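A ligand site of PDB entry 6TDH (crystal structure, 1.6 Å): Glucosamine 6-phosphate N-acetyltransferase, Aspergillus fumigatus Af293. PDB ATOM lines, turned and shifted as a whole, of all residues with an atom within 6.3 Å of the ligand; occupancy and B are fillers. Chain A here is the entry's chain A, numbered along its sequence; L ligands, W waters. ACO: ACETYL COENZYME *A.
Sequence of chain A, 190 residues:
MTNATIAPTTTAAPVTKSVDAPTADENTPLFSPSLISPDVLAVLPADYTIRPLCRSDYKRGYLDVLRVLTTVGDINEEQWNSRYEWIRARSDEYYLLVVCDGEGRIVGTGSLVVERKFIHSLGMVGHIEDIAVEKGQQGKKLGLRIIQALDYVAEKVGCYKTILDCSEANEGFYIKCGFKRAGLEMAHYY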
ATOM      1  N   VAL A  68     -18.658  -7.847 -10.492  1.00  0.00           N
ATOM      2  CA  VAL A  68     -19.911  -8.245  -9.780  1.00  0.00           C
ATOM      3  C   VAL A  68     -19.602  -9.043  -8.502  1.00  0.00           C
ATOM      4  O   VAL A  68     -20.460  -9.092  -7.600  1.00  0.00           O
ATOM      5  CB  VAL A  68     -20.825  -9.042 -10.728  1.00  0.00           C
ATOM      6  CG1 VAL A  68     -22.016  -9.645 -10.018  1.00  0.00           C
ATOM      7  CG2 VAL A  68     -21.265  -8.191 -11.921  1.00  0.00           C
ATOM      8  N   LEU A  69     -18.446  -9.690  -8.450  1.00  0.00           N
ATOM      9  CA  LEU A  69     -18.035 -10.683  -7.417  1.00  0.00           C
ATOM     10  C   LEU A  69     -17.247  -9.981  -6.322  1.00  0.00           C
ATOM     11  O   LEU A  69     -17.542 -10.228  -5.156  1.00  0.00           O
ATOM     12  CB  LEU A  69     -17.137 -11.732  -8.058  1.00  0.00           C
ATOM     13  CG  LEU A  69     -17.710 -13.134  -8.211  1.00  0.00           C
ATOM     14  CD1 LEU A  69     -16.660 -14.027  -8.828  1.00  0.00           C
ATOM     15  CD2 LEU A  69     -18.187 -13.677  -6.871  1.00  0.00           C
ATOM     16  N   ILE A 128     -17.315 -25.826  -7.922  1.00  0.00           N
ATOM     17  CA  ILE A 128     -17.845 -24.654  -8.660  1.00  0.00           C
ATOM     18  C   ILE A 128     -17.474 -23.370  -7.915  1.00  0.00           C
ATOM     19  O   ILE A 128     -17.660 -23.302  -6.676  1.00  0.00           O
ATOM     20  CB  ILE A 128     -19.331 -24.803  -8.992  1.00  0.00           C
ATOM     21  CG1 ILE A 128     -19.473 -25.854 -10.085  1.00  0.00           C
ATOM     22  CG2 ILE A 128     -19.950 -23.470  -9.396  1.00  0.00           C
ATOM     23  CD1 ILE A 128     -20.861 -26.219 -10.403  1.00  0.00           C
ATOM     24  N   GLU A 129     -16.944 -22.396  -8.650  1.00  0.00           N
ATOM     25  CA  GLU A 129     -16.411 -21.164  -8.032  1.00  0.00           C
ATOM     26  C   GLU A 129     -16.710 -19.954  -8.938  1.00  0.00           C
ATOM     27  O   GLU A 129     -16.766 -20.119 -10.179  1.00  0.00           O
ATOM     28  CB  GLU A 129     -14.896 -21.208  -7.845  1.00  0.00           C
ATOM     29  CG  GLU A 129     -14.351 -22.489  -7.250  1.00  0.00           C
ATOM     30  CD  GLU A 129     -14.520 -22.576  -5.751  1.00  0.00           C
ATOM     31  OE1 GLU A 129     -14.790 -21.522  -5.154  1.00  0.00           O
ATOM     32  OE2 GLU A 129     -14.406 -23.704  -5.194  1.00  0.00           O
ATOM     33  N   ASP A 130     -16.803 -18.797  -8.327  1.00  0.00           N
ATOM     34  CA  ASP A 130     -16.719 -17.517  -9.047  1.00  0.00           C
ATOM     35  C   ASP A 130     -17.754 -17.461 -10.190  1.00  0.00           C
ATOM     36  O   ASP A 130     -17.373 -17.022 -11.293  1.00  0.00           O
ATOM     37  CB  ASP A 130     -15.286 -17.305  -9.497  1.00  0.00           C
ATOM     38  CG  ASP A 130     -14.303 -17.232  -8.327  1.00  0.00           C
ATOM     39  OD1 ASP A 130     -14.738 -16.771  -7.275  1.00  0.00           O
ATOM     40  OD2 ASP A 130     -13.213 -17.733  -8.449  1.00  0.00           O
ATOM     41  N   ILE A 131     -19.016 -17.735  -9.869  1.00  0.00           N
ATOM     42  CA  ILE A 131     -20.143 -17.555 -10.825  1.00  0.00           C
ATOM     43  C   ILE A 131     -20.550 -16.076 -10.783  1.00  0.00           C
ATOM     44  O   ILE A 131     -20.775 -15.525  -9.671  1.00  0.00           O
ATOM     45  CB  ILE A 131     -21.333 -18.457 -10.506  1.00  0.00           C
ATOM     46  CG1 ILE A 131     -20.942 -19.937 -10.355  1.00  0.00           C
ATOM     47  CG2 ILE A 131     -22.429 -18.286 -11.566  1.00  0.00           C
ATOM     48  CD1 ILE A 131     -20.185 -20.478 -11.488  1.00  0.00           C
ATOM     49  N   ALA A 132     -20.639 -15.419 -11.935  1.00  0.00           N
ATOM     50  CA  ALA A 132     -21.052 -14.005 -11.957  1.00  0.00           C
ATOM     51  C   ALA A 132     -21.819 -13.749 -13.246  1.00  0.00           C
ATOM     52  O   ALA A 132     -21.344 -14.165 -14.337  1.00  0.00           O
ATOM     53  CB  ALA A 132     -19.894 -13.070 -11.781  1.00  0.00           C
ATOM     54  N   VAL A 133     -22.863 -12.947 -13.130  1.00  0.00           N
ATOM     55  CA  VAL A 133     -23.649 -12.504 -14.294  1.00  0.00           C
ATOM     56  C   VAL A 133     -23.748 -10.970 -14.176  1.00  0.00           C
ATOM     57  O   VAL A 133     -24.035 -10.502 -13.099  1.00  0.00           O
ATOM     58  CB  VAL A 133     -25.011 -13.187 -14.396  1.00  0.00           C
ATOM     59  CG1 VAL A 133     -25.882 -12.570 -15.484  1.00  0.00           C
ATOM     60  CG2 VAL A 133     -24.925 -14.687 -14.601  1.00  0.00           C
ATOM     61  N   GLU A 134     -23.445 -10.243 -15.245  1.00  0.00           N
ATOM     62  CA  GLU A 134     -23.583  -8.756 -15.253  1.00  0.00           C
ATOM     63  C   GLU A 134     -24.981  -8.378 -14.737  1.00  0.00           C
ATOM     64  O   GLU A 134     -25.969  -8.994 -15.139  1.00  0.00           O
ATOM     65  CB  GLU A 134     -23.306  -8.304 -16.688  1.00  0.00           C
ATOM     66  CG  GLU A 134     -23.809  -6.939 -17.079  1.00  0.00           C
ATOM     67  CD  GLU A 134     -23.504  -6.775 -18.562  1.00  0.00           C
ATOM     68  OE1 GLU A 134     -22.304  -6.816 -18.911  1.00  0.00           O
ATOM     69  OE2 GLU A 134     -24.458  -6.730 -19.354  1.00  0.00           O
ATOM     70  N   GLN A 137     -28.132  -8.356 -16.892  1.00  0.00           N
ATOM     71  CA  GLN A 137     -28.435  -9.635 -17.585  1.00  0.00           C
ATOM     72  C   GLN A 137     -28.833 -10.694 -16.551  1.00  0.00           C
ATOM     73  O   GLN A 137     -29.109 -11.831 -16.986  1.00  0.00           O
ATOM     74  CB  GLN A 137     -27.182 -10.125 -18.316  1.00  0.00           C
ATOM     75  CG  GLN A 137     -26.717  -9.184 -19.409  1.00  0.00           C
ATOM     76  CD  GLN A 137     -27.603  -9.358 -20.602  1.00  0.00           C
ATOM     77  OE1 GLN A 137     -27.512 -10.370 -21.288  1.00  0.00           O
ATOM     78  NE2 GLN A 137     -28.485  -8.403 -20.826  1.00  0.00           N
ATOM     79  N   GLN A 138     -28.929 -10.306 -15.281  1.00  0.00           N
ATOM     80  CA  GLN A 138     -29.341 -11.226 -14.173  1.00  0.00           C
ATOM     81  C   GLN A 138     -30.830 -11.516 -14.289  1.00  0.00           C
ATOM     82  O   GLN A 138     -31.585 -10.699 -14.916  1.00  0.00           O
ATOM     83  CB  GLN A 138     -28.998 -10.673 -12.806  1.00  0.00           C
ATOM     84  CG  GLN A 138     -27.532 -10.696 -12.505  1.00  0.00           C
ATOM     85  CD  GLN A 138     -27.203 -10.196 -11.131  1.00  0.00           C
ATOM     86  OE1 GLN A 138     -28.102  -9.990 -10.308  1.00  0.00           O
ATOM     87  NE2 GLN A 138     -25.922  -9.964 -10.913  1.00  0.00           N
ATOM     88  N   GLY A 139     -31.224 -12.693 -13.838  1.00  0.00           N
ATOM     89  CA  GLY A 139     -32.626 -13.118 -13.788  1.00  0.00           C
ATOM     90  C   GLY A 139     -33.181 -13.529 -15.123  1.00  0.00           C
ATOM     91  O   GLY A 139     -34.437 -13.510 -15.267  1.00  0.00           O
ATOM     92  N   LYS A 140     -32.312 -13.984 -16.044  1.00  0.00           N
ATOM     93  CA  LYS A 140     -32.676 -14.467 -17.383  1.00  0.00           C
ATOM     94  C   LYS A 140     -32.184 -15.896 -17.600  1.00  0.00           C
ATOM     95  O   LYS A 140     -32.096 -16.319 -18.779  1.00  0.00           O
ATOM     96  CB  LYS A 140     -32.062 -13.507 -18.417  1.00  0.00           C
ATOM     97  CG  LYS A 140     -32.440 -12.048 -18.253  1.00  0.00           C
ATOM     98  CD  LYS A 140     -32.443 -11.292 -19.590  1.00  0.00           C
ATOM     99  CE  LYS A 140     -32.920  -9.855 -19.485  1.00  0.00           C
ATOM    100  NZ  LYS A 140     -31.805  -8.889 -19.549  1.00  0.00           N
ATOM    101  N   LYS A 141     -31.802 -16.593 -16.523  1.00  0.00           N
ATOM    102  CA  LYS A 141     -31.377 -18.026 -16.532  1.00  0.00           C
ATOM    103  C   LYS A 141     -29.901 -18.180 -16.950  1.00  0.00           C
ATOM    104  O   LYS A 141     -29.495 -19.346 -17.075  1.00  0.00           O
ATOM    105  CB  LYS A 141     -32.249 -18.947 -17.390  1.00  0.00           C
ATOM    106  CG  LYS A 141     -33.757 -18.881 -17.098  1.00  0.00           C
ATOM    107  CD  LYS A 141     -34.193 -19.813 -16.019  1.00  0.00           C
ATOM    108  CE  LYS A 141     -35.677 -20.105 -16.014  1.00  0.00           C
ATOM    109  NZ  LYS A 141     -36.459 -18.875 -16.251  1.00  0.00           N
ATOM    110  N   LEU A 142     -29.147 -17.106 -17.120  1.00  0.00           N
ATOM    111  CA  LEU A 142     -27.726 -17.229 -17.548  1.00  0.00           C
ATOM    112  C   LEU A 142     -26.904 -17.880 -16.418  1.00  0.00           C
ATOM    113  O   LEU A 142     -26.070 -18.708 -16.719  1.00  0.00           O
ATOM    114  CB  LEU A 142     -27.145 -15.877 -17.902  1.00  0.00           C
ATOM    115  CG  LEU A 142     -27.808 -15.229 -19.136  1.00  0.00           C
ATOM    116  CD1 LEU A 142     -27.179 -13.907 -19.407  1.00  0.00           C
ATOM    117  CD2 LEU A 142     -27.774 -16.153 -20.336  1.00  0.00           C
ATOM    118  N   GLY A 143     -27.176 -17.560 -15.151  1.00  0.00           N
ATOM    119  CA  GLY A 143     -26.477 -18.266 -14.073  1.00  0.00           C
ATOM    120  C   GLY A 143     -26.814 -19.745 -14.072  1.00  0.00           C
ATOM    121  O   GLY A 143     -25.890 -20.592 -13.861  1.00  0.00           O
ATOM    122  N   LEU A 144     -28.085 -20.108 -14.241  1.00  0.00           N
ATOM    123  CA  LEU A 144     -28.476 -21.540 -14.366  1.00  0.00           C
ATOM    124  C   LEU A 144     -27.680 -22.187 -15.514  1.00  0.00           C
ATOM    125  O   LEU A 144     -27.203 -23.314 -15.357  1.00  0.00           O
ATOM    126  CB  LEU A 144     -29.981 -21.632 -14.584  1.00  0.00           C
ATOM    127  CG  LEU A 144     -30.522 -23.008 -14.927  1.00  0.00           C
ATOM    128  CD1 LEU A 144     -30.380 -23.996 -13.768  1.00  0.00           C
ATOM    129  CD2 LEU A 144     -32.013 -22.877 -15.310  1.00  0.00           C
ATOM    130  N   ARG A 145     -27.642 -21.549 -16.680  1.00  0.00           N
ATOM    131  CA  ARG A 145     -26.933 -22.131 -17.852  1.00  0.00           C
ATOM    132  C   ARG A 145     -25.450 -22.327 -17.502  1.00  0.00           C
ATOM    133  O   ARG A 145     -24.860 -23.323 -17.924  1.00  0.00           O
ATOM    134  CB  ARG A 145     -27.095 -21.250 -19.069  1.00  0.00           C
ATOM    135  CG  ARG A 145     -28.547 -21.099 -19.536  1.00  0.00           C
ATOM    136  CD  ARG A 145     -29.426 -22.300 -19.344  1.00  0.00           C
ATOM    137  NE  ARG A 145     -30.810 -22.027 -19.727  1.00  0.00           N
ATOM    138  CZ  ARG A 145     -31.823 -22.838 -19.459  1.00  0.00           C
ATOM    139  NH1 ARG A 145     -31.630 -23.969 -18.816  1.00  0.00           N
ATOM    140  NH2 ARG A 145     -33.060 -22.508 -19.825  1.00  0.00           N
ATOM    141  N   ILE A 146     -24.828 -21.350 -16.858  1.00  0.00           N
ATOM    142  CA  ILE A 146     -23.400 -21.473 -16.426  1.00  0.00           C
ATOM    143  C   ILE A 146     -23.235 -22.693 -15.528  1.00  0.00           C
ATOM    144  O   ILE A 146     -22.355 -23.491 -15.757  1.00  0.00           O
ATOM    145  CB  ILE A 146     -22.936 -20.191 -15.758  1.00  0.00           C
ATOM    146  CG1 ILE A 146     -22.892 -19.045 -16.770  1.00  0.00           C
ATOM    147  CG2 ILE A 146     -21.579 -20.385 -15.030  1.00  0.00           C
ATOM    148  CD1 ILE A 146     -22.814 -17.718 -16.130  1.00  0.00           C
ATOM    149  N   LEU A 164     -20.065 -26.858  -4.073  1.00  0.00           N
ATOM    150  CA  LEU A 164     -19.780 -25.411  -3.989  1.00  0.00           C
ATOM    151  C   LEU A 164     -20.200 -24.960  -2.588  1.00  0.00           C
ATOM    152  O   LEU A 164     -20.934 -25.662  -1.913  1.00  0.00           O
ATOM    153  CB  LEU A 164     -20.517 -24.634  -5.094  1.00  0.00           C
ATOM    154  CG  LEU A 164     -22.035 -24.797  -5.105  1.00  0.00           C
ATOM    155  CD1 LEU A 164     -22.734 -23.803  -4.165  1.00  0.00           C
ATOM    156  CD2 LEU A 164     -22.604 -24.676  -6.527  1.00  0.00           C
ATOM    157  N   ASP A 165     -19.707 -23.806  -2.190  1.00  0.00           N
ATOM    158  CA  ASP A 165     -20.092 -23.135  -0.943  1.00  0.00           C
ATOM    159  C   ASP A 165     -20.935 -21.934  -1.336  1.00  0.00           C
ATOM    160  O   ASP A 165     -20.568 -21.209  -2.306  1.00  0.00           O
ATOM    161  CB  ASP A 165     -18.855 -22.735  -0.170  1.00  0.00           C
ATOM    162  CG  ASP A 165     -18.058 -23.929   0.327  1.00  0.00           C
ATOM    163  OD1 ASP A 165     -18.666 -24.936   0.771  1.00  0.00           O
ATOM    164  OD2 ASP A 165     -16.834 -23.845   0.218  1.00  0.00           O
ATOM    165  N   CYS A 166     -21.962 -21.668  -0.571  1.00  0.00           N
ATOM    166  CA  CYS A 166     -22.791 -20.479  -0.846  1.00  0.00           C
ATOM    167  C   CYS A 166     -23.232 -19.862   0.485  1.00  0.00           C
ATOM    168  O   CYS A 166     -23.087 -20.495   1.525  1.00  0.00           O
ATOM    169  CB  CYS A 166     -23.939 -20.869  -1.752  1.00  0.00           C
ATOM    170  SG  CYS A 166     -25.193 -21.887  -0.958  1.00  0.00           S
ATOM    171  N   SER A 167     -23.693 -18.610   0.411  1.00  0.00           N
ATOM    172  CA  SER A 167     -24.376 -17.889   1.513  1.00  0.00           C
ATOM    173  C   SER A 167     -25.789 -18.460   1.637  1.00  0.00           C
ATOM    174  O   SER A 167     -26.278 -19.006   0.637  1.00  0.00           O
ATOM    175  CB  SER A 167     -24.427 -16.403   1.241  1.00  0.00           C
ATOM    176  OG  SER A 167     -25.162 -16.130   0.055  1.00  0.00           O
ATOM    177  N   ALA A 169     -28.294 -16.627   1.510  1.00  0.00           N
ATOM    178  CA  ALA A 169     -29.064 -15.709   0.618  1.00  0.00           C
ATOM    179  C   ALA A 169     -29.090 -16.218  -0.840  1.00  0.00           C
ATOM    180  O   ALA A 169     -30.061 -15.929  -1.562  1.00  0.00           O
ATOM    181  CB  ALA A 169     -28.475 -14.320   0.694  1.00  0.00           C
ATOM    182  N   ASN A 170     -28.087 -16.928  -1.334  1.00  0.00           N
ATOM    183  CA  ASN A 170     -28.194 -17.408  -2.737  1.00  0.00           C
ATOM    184  C   ASN A 170     -28.389 -18.928  -2.727  1.00  0.00           C
ATOM    185  O   ASN A 170     -28.385 -19.494  -3.826  1.00  0.00           O
ATOM    186  CB  ASN A 170     -27.117 -16.836  -3.654  1.00  0.00           C
ATOM    187  CG  ASN A 170     -25.706 -17.068  -3.160  1.00  0.00           C
ATOM    188  OD1 ASN A 170     -25.503 -17.925  -2.303  1.00  0.00           O
ATOM    189  ND2 ASN A 170     -24.749 -16.340  -3.717  1.00  0.00           N
ATOM    190  N   GLU A 171     -28.723 -19.539  -1.586  1.00  0.00           N
ATOM    191  CA  GLU A 171     -29.004 -20.993  -1.533  1.00  0.00           C
ATOM    192  C   GLU A 171     -30.093 -21.337  -2.549  1.00  0.00           C
ATOM    193  O   GLU A 171     -30.015 -22.372  -3.201  1.00  0.00           O
ATOM    194  CB  GLU A 171     -29.383 -21.504  -0.138  1.00  0.00           C
ATOM    195  CG  GLU A 171     -29.449 -23.007  -0.063  1.00  0.00           C
ATOM    196  CD  GLU A 171     -29.946 -23.631   1.232  1.00  0.00           C
ATOM    197  OE1 GLU A 171     -30.427 -22.913   2.085  1.00  0.00           O
ATOM    198  OE2 GLU A 171     -29.836 -24.870   1.359  1.00  0.00           O
ATOM    199  N   GLY A 172     -31.145 -20.530  -2.608  1.00  0.00           N
ATOM    200  CA  GLY A 172     -32.306 -20.821  -3.464  1.00  0.00           C
ATOM    201  C   GLY A 172     -31.929 -20.841  -4.924  1.00  0.00           C
ATOM    202  O   GLY A 172     -32.554 -21.617  -5.668  1.00  0.00           O
ATOM    203  N   PHE A 173     -30.927 -20.032  -5.320  1.00  0.00           N
ATOM    204  CA  PHE A 173     -30.365 -20.127  -6.695  1.00  0.00           C
ATOM    205  C   PHE A 173     -29.809 -21.543  -6.930  1.00  0.00           C
ATOM    206  O   PHE A 173     -30.227 -22.208  -7.868  1.00  0.00           O
ATOM    207  CB  PHE A 173     -29.291 -19.087  -6.937  1.00  0.00           C
ATOM    208  CG  PHE A 173     -28.532 -19.295  -8.220  1.00  0.00           C
ATOM    209  CD1 PHE A 173     -27.191 -19.612  -8.179  1.00  0.00           C
ATOM    210  CD2 PHE A 173     -29.175 -19.216  -9.452  1.00  0.00           C
ATOM    211  CE1 PHE A 173     -26.482 -19.790  -9.351  1.00  0.00           C
ATOM    212  CE2 PHE A 173     -28.469 -19.425 -10.621  1.00  0.00           C
ATOM    213  CZ  PHE A 173     -27.123 -19.735 -10.560  1.00  0.00           C
ATOM    214  N   TYR A 174     -28.953 -22.048  -6.044  1.00  0.00           N
ATOM    215  CA  TYR A 174     -28.348 -23.389  -6.229  1.00  0.00           C
ATOM    216  C   TYR A 174     -29.377 -24.496  -6.146  1.00  0.00           C
ATOM    217  O   TYR A 174     -29.227 -25.513  -6.838  1.00  0.00           O
ATOM    218  CB  TYR A 174     -27.154 -23.575  -5.286  1.00  0.00           C
ATOM    219  CG  TYR A 174     -26.105 -22.543  -5.544  1.00  0.00           C
ATOM    220  CD1 TYR A 174     -25.954 -21.479  -4.670  1.00  0.00           C
ATOM    221  CD2 TYR A 174     -25.344 -22.562  -6.706  1.00  0.00           C
ATOM    222  CE1 TYR A 174     -25.021 -20.493  -4.922  1.00  0.00           C
ATOM    223  CE2 TYR A 174     -24.420 -21.561  -6.971  1.00  0.00           C
ATOM    224  CZ  TYR A 174     -24.273 -20.529  -6.065  1.00  0.00           C
ATOM    225  OH  TYR A 174     -23.363 -19.519  -6.268  1.00  0.00           O
ATOM    226  N   LYS A 176     -32.458 -24.239  -7.268  1.00  0.00           N
ATOM    227  CA  LYS A 176     -33.064 -24.187  -8.628  1.00  0.00           C
ATOM    228  C   LYS A 176     -32.132 -24.842  -9.665  1.00  0.00           C
ATOM    229  O   LYS A 176     -32.664 -25.345 -10.677  1.00  0.00           O
ATOM    230  CB  LYS A 176     -33.411 -22.746  -8.978  1.00  0.00           C
ATOM    231  CG  LYS A 176     -34.597 -22.159  -8.208  1.00  0.00           C
ATOM    232  CD  LYS A 176     -35.929 -22.316  -8.913  1.00  0.00           C
ATOM    233  CE  LYS A 176     -37.154 -21.800  -8.148  1.00  0.00           C
ATOM    234  NZ  LYS A 176     -37.513 -20.401  -8.524  1.00  0.00           N
ATOM    235  N   CYS A 177     -30.815 -24.879  -9.439  1.00  0.00           N
ATOM    236  CA  CYS A 177     -29.834 -25.492 -10.370  1.00  0.00           C
ATOM    237  C   CYS A 177     -29.636 -26.976 -10.057  1.00  0.00           C
ATOM    238  O   CYS A 177     -28.766 -27.576 -10.708  1.00  0.00           O
ATOM    239  CB  CYS A 177     -28.473 -24.825 -10.315  1.00  0.00           C
ATOM    240  SG  CYS A 177     -28.430 -23.059 -10.707  1.00  0.00           S
HETATM  241  N1A ACO L   1     -32.242 -16.751  -4.413  1.00  0.00           N
HETATM  242  C2A ACO L   1     -33.257 -17.478  -4.881  1.00  0.00           C
HETATM  243  N3A ACO L   1     -33.502 -17.640  -6.200  1.00  0.00           N
HETATM  244  C4A ACO L   1     -32.649 -17.070  -7.095  1.00  0.00           C
HETATM  245  C5A ACO L   1     -31.548 -16.279  -6.658  1.00  0.00           C
HETATM  246  C6A ACO L   1     -31.348 -16.169  -5.223  1.00  0.00           C
HETATM  247  N6A ACO L   1     -30.318 -15.455  -4.734  1.00  0.00           N
HETATM  248  N7A ACO L   1     -30.872 -15.857  -7.738  1.00  0.00           N
HETATM  249  C8A ACO L   1     -31.526 -16.337  -8.795  1.00  0.00           C
HETATM  250  N9A ACO L   1     -32.616 -17.031  -8.432  1.00  0.00           N
HETATM  251  C1B ACO L   1     -33.520 -17.743  -9.316  1.00  0.00           C
HETATM  252  C2B ACO L   1     -33.888 -17.031 -10.576  1.00  0.00           C
HETATM  253  O2B ACO L   1     -34.968 -16.105 -10.361  1.00  0.00           O
HETATM  254  C3B ACO L   1     -34.369 -18.197 -11.432  1.00  0.00           C
HETATM  255  O3B ACO L   1     -35.607 -18.740 -10.972  1.00  0.00           O
HETATM  256  P3B ACO L   1     -36.680 -19.425 -12.029  1.00  0.00           P
HETATM  257  O7A ACO L   1     -36.066 -20.733 -12.470  1.00  0.00           O
HETATM  258  O8A ACO L   1     -37.841 -19.643 -11.130  1.00  0.00           O
HETATM  259  O9A ACO L   1     -36.703 -18.390 -13.059  1.00  0.00           O
HETATM  260  C4B ACO L   1     -33.352 -19.257 -11.067  1.00  0.00           C
HETATM  261  O4B ACO L   1     -32.902 -18.992  -9.745  1.00  0.00           O
HETATM  262  C5B ACO L   1     -32.145 -19.173 -12.000  1.00  0.00           C
HETATM  263  O5B ACO L   1     -31.470 -17.935 -11.806  1.00  0.00           O
HETATM  264  P1A ACO L   1     -30.735 -17.105 -12.992  1.00  0.00           P
HETATM  265  O1A ACO L   1     -31.787 -16.267 -13.724  1.00  0.00           O
HETATM  266  O2A ACO L   1     -29.895 -18.054 -13.821  1.00  0.00           O
HETATM  267  O3A ACO L   1     -29.845 -16.154 -12.147  1.00  0.00           O
HETATM  268  P2A ACO L   1     -28.766 -15.106 -12.466  1.00  0.00           P
HETATM  269  O4A ACO L   1     -29.111 -13.839 -11.804  1.00  0.00           O
HETATM  270  O5A ACO L   1     -28.467 -15.158 -13.956  1.00  0.00           O
HETATM  271  O6A ACO L   1     -27.469 -15.630 -11.747  1.00  0.00           O
HETATM  272  CBP ACO L   1     -26.153 -15.362  -9.868  1.00  0.00           C
HETATM  273  CCP ACO L   1     -27.426 -15.955 -10.346  1.00  0.00           C
HETATM  274  CDP ACO L   1     -24.975 -15.912 -10.688  1.00  0.00           C
HETATM  275  CEP ACO L   1     -26.096 -15.694  -8.366  1.00  0.00           C
HETATM  276  CAP ACO L   1     -26.150 -13.827 -10.111  1.00  0.00           C
HETATM  277  OAP ACO L   1     -27.275 -13.255  -9.440  1.00  0.00           O
HETATM  278  C9P ACO L   1     -24.917 -13.094  -9.675  1.00  0.00           C
HETATM  279  O9P ACO L   1     -23.979 -12.916 -10.412  1.00  0.00           O
HETATM  280  N8P ACO L   1     -24.799 -12.619  -8.389  1.00  0.00           N
HETATM  281  C7P ACO L   1     -23.635 -11.921  -7.937  1.00  0.00           C
HETATM  282  C6P ACO L   1     -22.339 -12.726  -7.779  1.00  0.00           C
HETATM  283  C5P ACO L   1     -22.502 -13.961  -6.890  1.00  0.00           C
HETATM  284  O5P ACO L   1     -22.971 -13.819  -5.764  1.00  0.00           O
HETATM  285  N4P ACO L   1     -22.111 -15.167  -7.355  1.00  0.00           N
HETATM  286  C3P ACO L   1     -22.110 -16.397  -6.550  1.00  0.00           C
HETATM  287  C2P ACO L   1     -20.771 -16.525  -5.808  1.00  0.00           C
HETATM  288  S1P ACO L   1     -20.753 -18.094  -4.976  1.00  0.00           S
HETATM  289  C   ACO L   1     -20.240 -19.207  -6.134  1.00  0.00           C
HETATM  290  O   ACO L   1     -19.953 -18.807  -7.252  1.00  0.00           O
HETATM  291  CH3 ACO L   1     -20.192 -20.668  -5.788  1.00  0.00           C
HETATM  292  O   HOH W   1     -29.165 -13.690  -7.398  1.00  0.00           O
HETATM  293  O   HOH W   2     -26.359 -12.841  -5.809  1.00  0.00           O
HETATM  294  O   HOH W   3     -31.076 -13.181 -10.280  1.00  0.00           O
HETATM  295  O   HOH W   4     -17.987 -19.830  -3.350  1.00  0.00           O
HETATM  296  O   HOH W   5     -33.964 -13.470 -10.344  1.00  0.00           O
HETATM  297  O   HOH W   6     -32.326 -17.645  -1.857  1.00  0.00           O
HETATM  298  O   HOH W   7     -34.291 -16.028 -13.792  1.00  0.00           O
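The backbone NH (N) of Ile 131 sits at hydrogen-bond distance from an oxygen (O) of the ligand, at 3.0 Å.
The backbone carbonyl oxygen (O) of Ile 131 is in hydrogen-bond range of a nitrogen (N4P) of the ligand (2.7 Å).
The side-chain amino group (NZ) of Lys 176 is in salt-bridge range of an oxygen (O8A) of the ligand.
An oxygen (O2A) of the ligand sits at hydrogen-bond distance from the backbone NH of Leu 144 (2.8 Å).
The backbone NH (N) of Lys 141 sits at hydrogen-bond distance from an oxygen (O1A) of the ligand (2.8 Å).
NZ of Lys 141 lies within salt-bridge range of O9A of the ligand.
N of Val 133 lies within hydrogen-bond range of O9P of the ligand.
The backbone NH of Gly 143 is in hydrogen-bond range of an oxygen (O5A) of the ligand.
A sulfur (S1P) of the ligand sits close to the side-chain hydroxyl (OH) of Tyr 174, 3.2 Å away.
N of Gly 139 sits at hydrogen-bond distance from O4A of the ligand (3.1 Å).
The backbone carbonyl oxygen (O) of Ala 169 is in hydrogen-bond range of a nitrogen (N6A) of the ligand, at 3.2 Å.
The backbone NH (N) of Lys 140 lies within hydrogen-bond range of an oxygen (O1A) of the ligand.
The side-chain amide oxygen of Gln 138 is in hydrogen-bond range of an oxygen (OAP) of the ligand, 3.5 Å away.
N of Asp 130 lies within hydrogen-bond range of O of the ligand (3.3 Å).
The backbone carbonyl oxygen (O) of Val 133 lies within hydrogen-bond range of the side-chain amide nitrogen (NE2) of Gln 138 (2.9 Å).
The side-chain hydroxyl (OG) of Ser 167 sits close to the backbone NH (N) of Ala 169.
The side-chain sulfur (SG) of Cys 177 is in hydrogen-bond range of the backbone carbonyl oxygen (O) of Phe 173 (3.5 Å).
OG of Ser 167 sits at hydrogen-bond distance from OD1 of Asn 170 (3.0 Å).
Merely in contact with the ligand: Val 68 (3.5 Å), Leu 69 (3.99 Å), Ile 128 (3.8 Å), Glu 129 (3.8 Å), Ala 132 (3.5 Å), Leu 142 (3.5 Å), Asp 165 (3.5 Å), Asn 170 (3.5 Å), Gly 172 (3.6 Å) and Phe 173 (3.5 Å).
Hydrophobic or aromatic side chains within 4 Å of the ligand: Val 68, Leu 69, Ile 131, Val 133, Leu 144 and Phe 173.
22 residues have an atom within 4 Å of the ligand: Val 68, Leu 69, Ile 128, Glu 129, Asp 130, Ile 131, Ala 132, Val 133, Gln 138, Gly 139, Lys 140, Lys 141, Leu 142, Gly 143, Leu 144, Asp 165, Ala 169, Asn 170, Gly 172, Phe 173, Tyr 174 and Lys 176.
The nearest printed residue that does not touch the ligand is Leu 164 (4.04 Å).
Water W7 lies within hydrogen-bond range of an oxygen (O1A) of the ligand (2.5 Å) and the backbone carbonyl oxygen of Gly 139 (2.9 Å).
Water W6 lies within hydrogen-bond range of a nitrogen (N1A) of the ligand (2.7 Å), the backbone carbonyl oxygen of Ala 169 (2.9 Å) and the backbone NH of Gly 172 (3.2 Å).
Water W4 lies within hydrogen-bond range of the backbone carbonyl oxygen (O) of Asp 165 (3.1 Å) and a sulfur (S1P) of the ligand (3.6 Å).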
